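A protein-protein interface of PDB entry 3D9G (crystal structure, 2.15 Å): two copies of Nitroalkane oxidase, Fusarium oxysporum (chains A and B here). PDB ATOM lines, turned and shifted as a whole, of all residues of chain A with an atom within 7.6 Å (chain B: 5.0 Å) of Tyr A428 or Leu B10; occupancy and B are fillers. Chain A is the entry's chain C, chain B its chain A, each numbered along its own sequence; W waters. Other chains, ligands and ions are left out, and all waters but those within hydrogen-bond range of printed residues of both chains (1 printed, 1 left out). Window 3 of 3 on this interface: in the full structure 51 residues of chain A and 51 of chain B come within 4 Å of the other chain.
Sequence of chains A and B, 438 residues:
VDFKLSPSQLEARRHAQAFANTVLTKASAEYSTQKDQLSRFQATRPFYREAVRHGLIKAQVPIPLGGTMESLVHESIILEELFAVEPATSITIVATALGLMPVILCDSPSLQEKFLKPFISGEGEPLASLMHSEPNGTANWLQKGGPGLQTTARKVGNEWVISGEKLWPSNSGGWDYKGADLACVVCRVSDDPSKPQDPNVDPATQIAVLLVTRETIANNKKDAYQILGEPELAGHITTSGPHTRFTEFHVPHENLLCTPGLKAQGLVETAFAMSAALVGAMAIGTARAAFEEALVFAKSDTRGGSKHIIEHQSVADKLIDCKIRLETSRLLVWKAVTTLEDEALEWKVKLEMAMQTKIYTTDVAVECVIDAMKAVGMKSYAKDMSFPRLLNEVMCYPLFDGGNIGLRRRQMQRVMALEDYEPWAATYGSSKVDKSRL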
ATOM      1  N   LYS A 335      14.661  -3.003  34.520  1.00  0.00           N
ATOM      2  CA  LYS A 335      14.564  -2.634  33.114  1.00  0.00           C
ATOM      3  C   LYS A 335      13.642  -3.589  32.319  1.00  0.00           C
ATOM      4  O   LYS A 335      12.805  -3.128  31.524  1.00  0.00           O
ATOM      5  CB  LYS A 335      15.955  -2.565  32.470  1.00  0.00           C
ATOM      6  CG  LYS A 335      15.953  -2.257  30.960  1.00  0.00           C
ATOM      7  CD  LYS A 335      15.202  -0.941  30.660  1.00  0.00           C
ATOM      8  CE  LYS A 335      15.386  -0.495  29.216  1.00  0.00           C
ATOM      9  NZ  LYS A 335      14.784   0.865  29.027  1.00  0.00           N
ATOM     10  N   LEU A 345       5.823  -0.545  23.088  1.00  0.00           N
ATOM     11  CA  LEU A 345       6.881  -1.353  22.470  1.00  0.00           C
ATOM     12  C   LEU A 345       6.313  -2.627  21.892  1.00  0.00           C
ATOM     13  O   LEU A 345       5.388  -3.219  22.456  1.00  0.00           O
ATOM     14  CB  LEU A 345       7.990  -1.682  23.484  1.00  0.00           C
ATOM     15  CG  LEU A 345       8.746  -0.493  24.082  1.00  0.00           C
ATOM     16  CD1 LEU A 345       9.560  -0.919  25.297  1.00  0.00           C
ATOM     17  CD2 LEU A 345       9.628   0.211  23.011  1.00  0.00           C
ATOM     18  N   PRO A 423      18.077  -3.101  18.000  1.00  0.00           N
ATOM     19  CA  PRO A 423      18.782  -3.400  19.248  1.00  0.00           C
ATOM     20  C   PRO A 423      18.434  -2.505  20.452  1.00  0.00           C
ATOM     21  O   PRO A 423      18.320  -3.011  21.578  1.00  0.00           O
ATOM     22  CB  PRO A 423      20.270  -3.268  18.862  1.00  0.00           C
ATOM     23  CG  PRO A 423      20.289  -2.627  17.513  1.00  0.00           C
ATOM     24  CD  PRO A 423      19.007  -2.991  16.860  1.00  0.00           C
ATOM     25  N   TRP A 424      18.242  -1.206  20.213  1.00  0.00           N
ATOM     26  CA  TRP A 424      18.099  -0.228  21.308  1.00  0.00           C
ATOM     27  C   TRP A 424      16.694   0.305  21.478  1.00  0.00           C
ATOM     28  O   TRP A 424      16.481   1.296  22.202  1.00  0.00           O
ATOM     29  CB  TRP A 424      19.110   0.923  21.150  1.00  0.00           C
ATOM     30  CG  TRP A 424      20.479   0.389  20.870  1.00  0.00           C
ATOM     31  CD1 TRP A 424      21.214   0.576  19.740  1.00  0.00           C
ATOM     32  CD2 TRP A 424      21.236  -0.488  21.706  1.00  0.00           C
ATOM     33  NE1 TRP A 424      22.394  -0.112  19.828  1.00  0.00           N
ATOM     34  CE2 TRP A 424      22.435  -0.777  21.024  1.00  0.00           C
ATOM     35  CE3 TRP A 424      21.016  -1.063  22.963  1.00  0.00           C
ATOM     36  CZ2 TRP A 424      23.425  -1.611  21.560  1.00  0.00           C
ATOM     37  CZ3 TRP A 424      22.004  -1.899  23.497  1.00  0.00           C
ATOM     38  CH2 TRP A 424      23.196  -2.151  22.797  1.00  0.00           C
ATOM     39  N   ALA A 425      15.731  -0.363  20.843  1.00  0.00           N
ATOM     40  CA  ALA A 425      14.345   0.110  20.873  1.00  0.00           C
ATOM     41  C   ALA A 425      13.742   0.260  22.279  1.00  0.00           C
ATOM     42  O   ALA A 425      12.914   1.146  22.489  1.00  0.00           O
ATOM     43  CB  ALA A 425      13.450  -0.757  19.981  1.00  0.00           C
ATOM     44  N   ALA A 426      14.155  -0.589  23.227  1.00  0.00           N
ATOM     45  CA  ALA A 426      13.676  -0.513  24.632  1.00  0.00           C
ATOM     46  C   ALA A 426      14.255   0.678  25.418  1.00  0.00           C
ATOM     47  O   ALA A 426      13.830   0.986  26.541  1.00  0.00           O
ATOM     48  CB  ALA A 426      13.980  -1.808  25.371  1.00  0.00           C
ATOM     49  N   THR A 427      15.227   1.343  24.813  1.00  0.00           N
ATOM     50  CA  THR A 427      15.959   2.411  25.472  1.00  0.00           C
ATOM     51  C   THR A 427      15.669   3.745  24.804  1.00  0.00           C
ATOM     52  O   THR A 427      15.217   4.678  25.456  1.00  0.00           O
ATOM     53  CB  THR A 427      17.477   2.113  25.450  1.00  0.00           C
ATOM     54  OG1 THR A 427      17.715   0.884  26.141  1.00  0.00           O
ATOM     55  CG2 THR A 427      18.280   3.224  26.102  1.00  0.00           C
ATOM     56  N   TYR A 428      15.918   3.799  23.499  1.00  0.00           N
ATOM     57  CA  TYR A 428      15.909   5.034  22.730  1.00  0.00           C
ATOM     58  C   TYR A 428      14.664   5.174  21.845  1.00  0.00           C
ATOM     59  O   TYR A 428      14.493   6.189  21.159  1.00  0.00           O
ATOM     60  CB  TYR A 428      17.207   5.150  21.907  1.00  0.00           C
ATOM     61  CG  TYR A 428      18.449   5.380  22.763  1.00  0.00           C
ATOM     62  CD1 TYR A 428      19.586   4.566  22.642  1.00  0.00           C
ATOM     63  CD2 TYR A 428      18.475   6.404  23.713  1.00  0.00           C
ATOM     64  CE1 TYR A 428      20.732   4.785  23.450  1.00  0.00           C
ATOM     65  CE2 TYR A 428      19.604   6.639  24.511  1.00  0.00           C
ATOM     66  CZ  TYR A 428      20.732   5.833  24.382  1.00  0.00           C
ATOM     67  OH  TYR A 428      21.833   6.102  25.195  1.00  0.00           O
ATOM     68  N   GLY A 429      13.787   4.167  21.903  1.00  0.00           N
ATOM     69  CA  GLY A 429      12.555   4.139  21.122  1.00  0.00           C
ATOM     70  C   GLY A 429      12.732   3.528  19.743  1.00  0.00           C
ATOM     71  O   GLY A 429      13.858   3.286  19.297  1.00  0.00           O
ATOM     72  N   SER A 430      11.608   3.277  19.069  1.00  0.00           N
ATOM     73  CA  SER A 430      11.611   2.740  17.705  1.00  0.00           C
ATOM     74  C   SER A 430      11.775   3.856  16.674  1.00  0.00           C
ATOM     75  O   SER A 430      12.439   3.671  15.644  1.00  0.00           O
ATOM     76  CB  SER A 430      10.330   1.946  17.435  1.00  0.00           C
ATOM     77  OG  SER A 430      10.289   1.451  16.104  1.00  0.00           O
ATOM     78  N   LEU B   5      12.675   8.237  28.356  1.00  0.00           N
ATOM     79  CA  LEU B   5      13.422   9.451  28.055  1.00  0.00           C
ATOM     80  C   LEU B   5      12.487  10.600  27.725  1.00  0.00           C
ATOM     81  O   LEU B   5      11.436  10.398  27.104  1.00  0.00           O
ATOM     82  CB  LEU B   5      14.386   9.228  26.889  1.00  0.00           C
ATOM     83  CG  LEU B   5      15.498   8.182  27.006  1.00  0.00           C
ATOM     84  CD1 LEU B   5      16.370   8.287  25.773  1.00  0.00           C
ATOM     85  CD2 LEU B   5      16.329   8.357  28.277  1.00  0.00           C
ATOM     86  N   SER B   6      12.886  11.800  28.140  1.00  0.00           N
ATOM     87  CA  SER B   6      12.106  13.005  27.906  1.00  0.00           C
ATOM     88  C   SER B   6      12.411  13.553  26.517  1.00  0.00           C
ATOM     89  O   SER B   6      13.362  13.104  25.865  1.00  0.00           O
ATOM     90  CB  SER B   6      12.405  14.053  28.990  1.00  0.00           C
ATOM     91  OG  SER B   6      13.767  14.438  28.974  1.00  0.00           O
ATOM     92  N   PRO B   7      11.590  14.508  26.031  1.00  0.00           N
ATOM     93  CA  PRO B   7      11.952  15.183  24.779  1.00  0.00           C
ATOM     94  C   PRO B   7      13.363  15.812  24.778  1.00  0.00           C
ATOM     95  O   PRO B   7      14.052  15.731  23.762  1.00  0.00           O
ATOM     96  CB  PRO B   7      10.868  16.255  24.640  1.00  0.00           C
ATOM     97  CG  PRO B   7       9.697  15.690  25.376  1.00  0.00           C
ATOM     98  CD  PRO B   7      10.286  14.972  26.549  1.00  0.00           C
ATOM     99  N   SER B   8      13.783  16.414  25.896  1.00  0.00           N
ATOM    100  CA  SER B   8      15.120  17.038  25.984  1.00  0.00           C
ATOM    101  C   SER B   8      16.248  15.996  25.972  1.00  0.00           C
ATOM    102  O   SER B   8      17.290  16.212  25.348  1.00  0.00           O
ATOM    103  CB  SER B   8      15.246  17.971  27.197  1.00  0.00           C
ATOM    104  OG  SER B   8      15.264  17.258  28.421  1.00  0.00           O
ATOM    105  N   GLN B   9      16.022  14.867  26.639  1.00  0.00           N
ATOM    106  CA  GLN B   9      16.945  13.730  26.573  1.00  0.00           C
ATOM    107  C   GLN B   9      17.017  13.155  25.159  1.00  0.00           C
ATOM    108  O   GLN B   9      18.102  12.910  24.632  1.00  0.00           O
ATOM    109  CB  GLN B   9      16.566  12.671  27.616  1.00  0.00           C
ATOM    110  CG  GLN B   9      17.112  13.007  29.002  1.00  0.00           C
ATOM    111  CD  GLN B   9      16.366  12.355  30.135  1.00  0.00           C
ATOM    112  OE1 GLN B   9      15.321  11.738  29.941  1.00  0.00           O
ATOM    113  NE2 GLN B   9      16.891  12.508  31.347  1.00  0.00           N
ATOM    114  N   LEU B  10      15.865  12.987  24.520  1.00  0.00           N
ATOM    115  CA  LEU B  10      15.838  12.559  23.120  1.00  0.00           C
ATOM    116  C   LEU B  10      16.462  13.584  22.163  1.00  0.00           C
ATOM    117  O   LEU B  10      17.108  13.212  21.179  1.00  0.00           O
ATOM    118  CB  LEU B  10      14.414  12.175  22.698  1.00  0.00           C
ATOM    119  CG  LEU B  10      13.847  10.897  23.335  1.00  0.00           C
ATOM    120  CD1 LEU B  10      12.324  10.878  23.240  1.00  0.00           C
ATOM    121  CD2 LEU B  10      14.437   9.620  22.716  1.00  0.00           C
ATOM    122  N   GLU B  11      16.289  14.872  22.448  1.00  0.00           N
ATOM    123  CA  GLU B  11      16.917  15.908  21.619  1.00  0.00           C
ATOM    124  C   GLU B  11      18.443  15.919  21.783  1.00  0.00           C
ATOM    125  O   GLU B  11      19.177  16.091  20.793  1.00  0.00           O
ATOM    126  CB  GLU B  11      16.296  17.296  21.886  1.00  0.00           C
ATOM    127  CG  GLU B  11      17.049  18.509  21.271  1.00  0.00           C
ATOM    128  CD  GLU B  11      17.184  18.467  19.748  1.00  0.00           C
ATOM    129  OE1 GLU B  11      18.067  19.187  19.212  1.00  0.00           O
ATOM    130  OE2 GLU B  11      16.415  17.727  19.079  1.00  0.00           O
ATOM    131  N   ALA B  12      18.916  15.723  23.016  1.00  0.00           N
ATOM    132  CA  ALA B  12      20.355  15.656  23.285  1.00  0.00           C
ATOM    133  C   ALA B  12      21.013  14.533  22.479  1.00  0.00           C
ATOM    134  O   ALA B  12      22.101  14.716  21.910  1.00  0.00           O
ATOM    135  CB  ALA B  12      20.625  15.494  24.773  1.00  0.00           C
ATOM    136  N   ARG B  13      20.336  13.384  22.415  1.00  0.00           N
ATOM    137  CA  ARG B  13      20.799  12.273  21.591  1.00  0.00           C
ATOM    138  C   ARG B  13      20.845  12.642  20.107  1.00  0.00           C
ATOM    139  O   ARG B  13      21.884  12.496  19.454  1.00  0.00           O
ATOM    140  CB  ARG B  13      19.923  11.032  21.799  1.00  0.00           C
ATOM    141  CG  ARG B  13      20.447   9.825  21.026  1.00  0.00           C
ATOM    142  CD  ARG B  13      19.657   8.561  21.255  1.00  0.00           C
ATOM    143  NE  ARG B  13      20.432   7.444  20.723  1.00  0.00           N
ATOM    144  CZ  ARG B  13      20.050   6.642  19.730  1.00  0.00           C
ATOM    145  NH1 ARG B  13      18.846   6.785  19.161  1.00  0.00           N
ATOM    146  NH2 ARG B  13      20.868   5.665  19.335  1.00  0.00           N
ATOM    147  N   ARG B  14      19.715  13.120  19.580  1.00  0.00           N
ATOM    148  CA  ARG B  14      19.639  13.567  18.187  1.00  0.00           C
ATOM    149  C   ARG B  14      20.732  14.589  17.854  1.00  0.00           C
ATOM    150  O   ARG B  14      21.415  14.454  16.843  1.00  0.00           O
ATOM    151  CB  ARG B  14      18.244  14.138  17.871  1.00  0.00           C
ATOM    152  CG  ARG B  14      18.070  14.581  16.409  1.00  0.00           C
ATOM    153  CD  ARG B  14      17.224  15.869  16.270  1.00  0.00           C
ATOM    154  NE  ARG B  14      17.890  17.070  16.799  1.00  0.00           N
ATOM    155  CZ  ARG B  14      18.881  17.717  16.184  1.00  0.00           C
ATOM    156  NH1 ARG B  14      19.342  17.282  15.010  1.00  0.00           N
ATOM    157  NH2 ARG B  14      19.419  18.798  16.746  1.00  0.00           N
ATOM    158  N   ILE B  77      24.165  10.236  27.713  1.00  0.00           N
ATOM    159  CA  ILE B  77      23.605  10.030  26.383  1.00  0.00           C
ATOM    160  C   ILE B  77      24.466  10.718  25.340  1.00  0.00           C
ATOM    161  O   ILE B  77      24.777  10.134  24.298  1.00  0.00           O
ATOM    162  CB  ILE B  77      22.139  10.522  26.318  1.00  0.00           C
ATOM    163  CG1 ILE B  77      21.239   9.613  27.173  1.00  0.00           C
ATOM    164  CG2 ILE B  77      21.648  10.572  24.882  1.00  0.00           C
ATOM    165  CD1 ILE B  77      19.862  10.184  27.501  1.00  0.00           C
ATOM    166  N   GLU B  80      27.878   8.798  24.864  1.00  0.00           N
ATOM    167  CA  GLU B  80      27.719   7.508  24.187  1.00  0.00           C
ATOM    168  C   GLU B  80      27.693   7.685  22.673  1.00  0.00           C
ATOM    169  O   GLU B  80      28.372   6.951  21.934  1.00  0.00           O
ATOM    170  CB  GLU B  80      26.459   6.768  24.651  1.00  0.00           C
ATOM    171  CG  GLU B  80      26.235   5.469  23.867  1.00  0.00           C
ATOM    172  CD  GLU B  80      25.132   4.606  24.414  1.00  0.00           C
ATOM    173  OE1 GLU B  80      24.666   3.712  23.681  1.00  0.00           O
ATOM    174  OE2 GLU B  80      24.728   4.818  25.569  1.00  0.00           O
ATOM    175  N   GLU B  81      26.929   8.681  22.221  1.00  0.00           N
ATOM    176  CA  GLU B  81      26.763   8.936  20.787  1.00  0.00           C
ATOM    177  C   GLU B  81      28.035   9.410  20.131  1.00  0.00           C
ATOM    178  O   GLU B  81      28.353   9.009  19.012  1.00  0.00           O
ATOM    179  CB  GLU B  81      25.611   9.922  20.528  1.00  0.00           C
ATOM    180  CG  GLU B  81      24.230   9.360  20.871  1.00  0.00           C
ATOM    181  CD  GLU B  81      23.952   8.023  20.183  1.00  0.00           C
ATOM    182  OE1 GLU B  81      24.355   7.852  19.004  1.00  0.00           O
ATOM    183  OE2 GLU B  81      23.331   7.143  20.812  1.00  0.00           O
ATOM    184  N   ARG B 288      29.843  -0.300  21.576  1.00  0.00           N
ATOM    185  CA  ARG B 288      28.622  -0.291  20.768  1.00  0.00           C
ATOM    186  C   ARG B 288      28.941  -0.277  19.289  1.00  0.00           C
ATOM    187  O   ARG B 288      28.274  -0.951  18.502  1.00  0.00           O
ATOM    188  CB  ARG B 288      27.748   0.932  21.078  1.00  0.00           C
ATOM    189  CG  ARG B 288      26.346   0.819  20.510  1.00  0.00           C
ATOM    190  CD  ARG B 288      25.483   2.023  20.872  1.00  0.00           C
ATOM    191  NE  ARG B 288      25.424   3.007  19.790  1.00  0.00           N
ATOM    192  CZ  ARG B 288      24.902   4.234  19.897  1.00  0.00           C
ATOM    193  NH1 ARG B 288      24.383   4.674  21.042  1.00  0.00           N
ATOM    194  NH2 ARG B 288      24.922   5.036  18.847  1.00  0.00           N
ATOM    195  N   ARG B 330      24.916   0.303  30.427  1.00  0.00           N
ATOM    196  CA  ARG B 330      24.173   1.583  30.363  1.00  0.00           C
ATOM    197  C   ARG B 330      23.243   1.743  31.539  1.00  0.00           C
ATOM    198  O   ARG B 330      23.125   2.823  32.090  1.00  0.00           O
ATOM    199  CB  ARG B 330      23.380   1.733  29.049  1.00  0.00           C
ATOM    200  CG  ARG B 330      23.005   3.189  28.669  1.00  0.00           C
ATOM    201  CD  ARG B 330      22.623   3.315  27.191  1.00  0.00           C
ATOM    202  NE  ARG B 330      21.954   2.091  26.819  1.00  0.00           N
ATOM    203  CZ  ARG B 330      22.247   1.312  25.789  1.00  0.00           C
ATOM    204  NH1 ARG B 330      23.164   1.639  24.887  1.00  0.00           N
ATOM    205  NH2 ARG B 330      21.559   0.209  25.668  1.00  0.00           N
ATOM    206  N   TRP B 334      23.533   4.952  34.169  1.00  0.00           N
ATOM    207  CA  TRP B 334      22.375   5.805  34.458  1.00  0.00           C
ATOM    208  C   TRP B 334      21.997   5.704  35.931  1.00  0.00           C
ATOM    209  O   TRP B 334      21.630   6.708  36.548  1.00  0.00           O
ATOM    210  CB  TRP B 334      21.205   5.488  33.510  1.00  0.00           C
ATOM    211  CG  TRP B 334      21.483   5.860  32.058  1.00  0.00           C
ATOM    212  CD1 TRP B 334      22.673   6.269  31.531  1.00  0.00           C
ATOM    213  CD2 TRP B 334      20.555   5.819  30.957  1.00  0.00           C
ATOM    214  NE1 TRP B 334      22.547   6.492  30.171  1.00  0.00           N
ATOM    215  CE2 TRP B 334      21.256   6.228  29.799  1.00  0.00           C
ATOM    216  CE3 TRP B 334      19.199   5.481  30.839  1.00  0.00           C
ATOM    217  CZ2 TRP B 334      20.640   6.323  28.534  1.00  0.00           C
ATOM    218  CZ3 TRP B 334      18.593   5.567  29.574  1.00  0.00           C
ATOM    219  CH2 TRP B 334      19.314   5.985  28.447  1.00  0.00           C
HETATM  220  O   HOH W   1      12.342   6.298  25.752  1.00  0.00           O
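The side-chain carboxylate (OE1) of Glu B80 lies within salt-bridge range of the guanidinium group (NH1) of Arg B330 (2.8 Å).
NH1 of Arg B288 is in salt-bridge range of OE2 of Glu B81, at 2.7 Å.
The side-chain carboxylate of Glu B80 is in salt-bridge range of the guanidinium group of Arg B288 (2.8 Å).
NE of Arg B13 lies within salt-bridge range of OE2 of Glu B81 (2.9 Å).
The side-chain hydroxyl (OH) of Tyr A428 lies within hydrogen-bond range of the side-chain carboxylate (OE2) of Glu B80 (3.2 Å).
Of chain B, only Leu B5 (3.5 Å), Leu B10 (3.8 Å), Arg B13 (3.5 Å), Glu B80 (3.2 Å), Arg B330 (3.5 Å) and Trp B334 (3.6 Å) come within 4 Å of Tyr A428.
Leu B10 touches just one residue of chain A: Tyr A428.
Of the printed residues of chain A, Glu B80 touches Tyr A428 (3.2 Å).
Of the printed residues of chain A, Trp B334 touches Thr A427 and Tyr A428.
Gln B9 touches none of the printed residues of chain A.
The nearest residue of chain B that does not touch Tyr A428 is Ile B77 (4.1 Å).
The nearest residue of chain A that does not touch Leu B10 is Gly A429 (5.6 Å).
Of the 10 printed residues of chain A, 3 touch a printed residue of chain B.
Along chain A the printed residues that touch a printed residue of chain B span positions 424 to 428.
No position is printed for both chains.
Of the 11 pairs that touch across the chains among the printed residues, none has its exchanged pair printed and touching as well.
CD of Arg B288 touches NE1 of Trp A424, at 3.9 Å.
Trp A424 touches Arg B330 (CE3 to NH2, 3.0 Å).
Thr A427 touches Leu B5 (O to CD1, 3.8 Å).
Thr A427 touches Arg B330 (CG2 to NE, 3.9 Å).
Thr A427 touches Trp B334 (CG2 to CH2, 3.8 Å).
Leu B5 touches Tyr A428 (CD1 to CD2, 3.5 Å).
CD2 of Leu B10 touches O of Tyr A428, 3.8 Å away.
Tyr A428 touches Arg B13.
Arg B330 touches Tyr A428 (CD to OH, 3.5 Å).
Tyr A428 touches Trp B334.
Water W1 lies within hydrogen-bond range of the backbone NH of Leu B5 and the backbone carbonyl oxygen of Thr A427.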
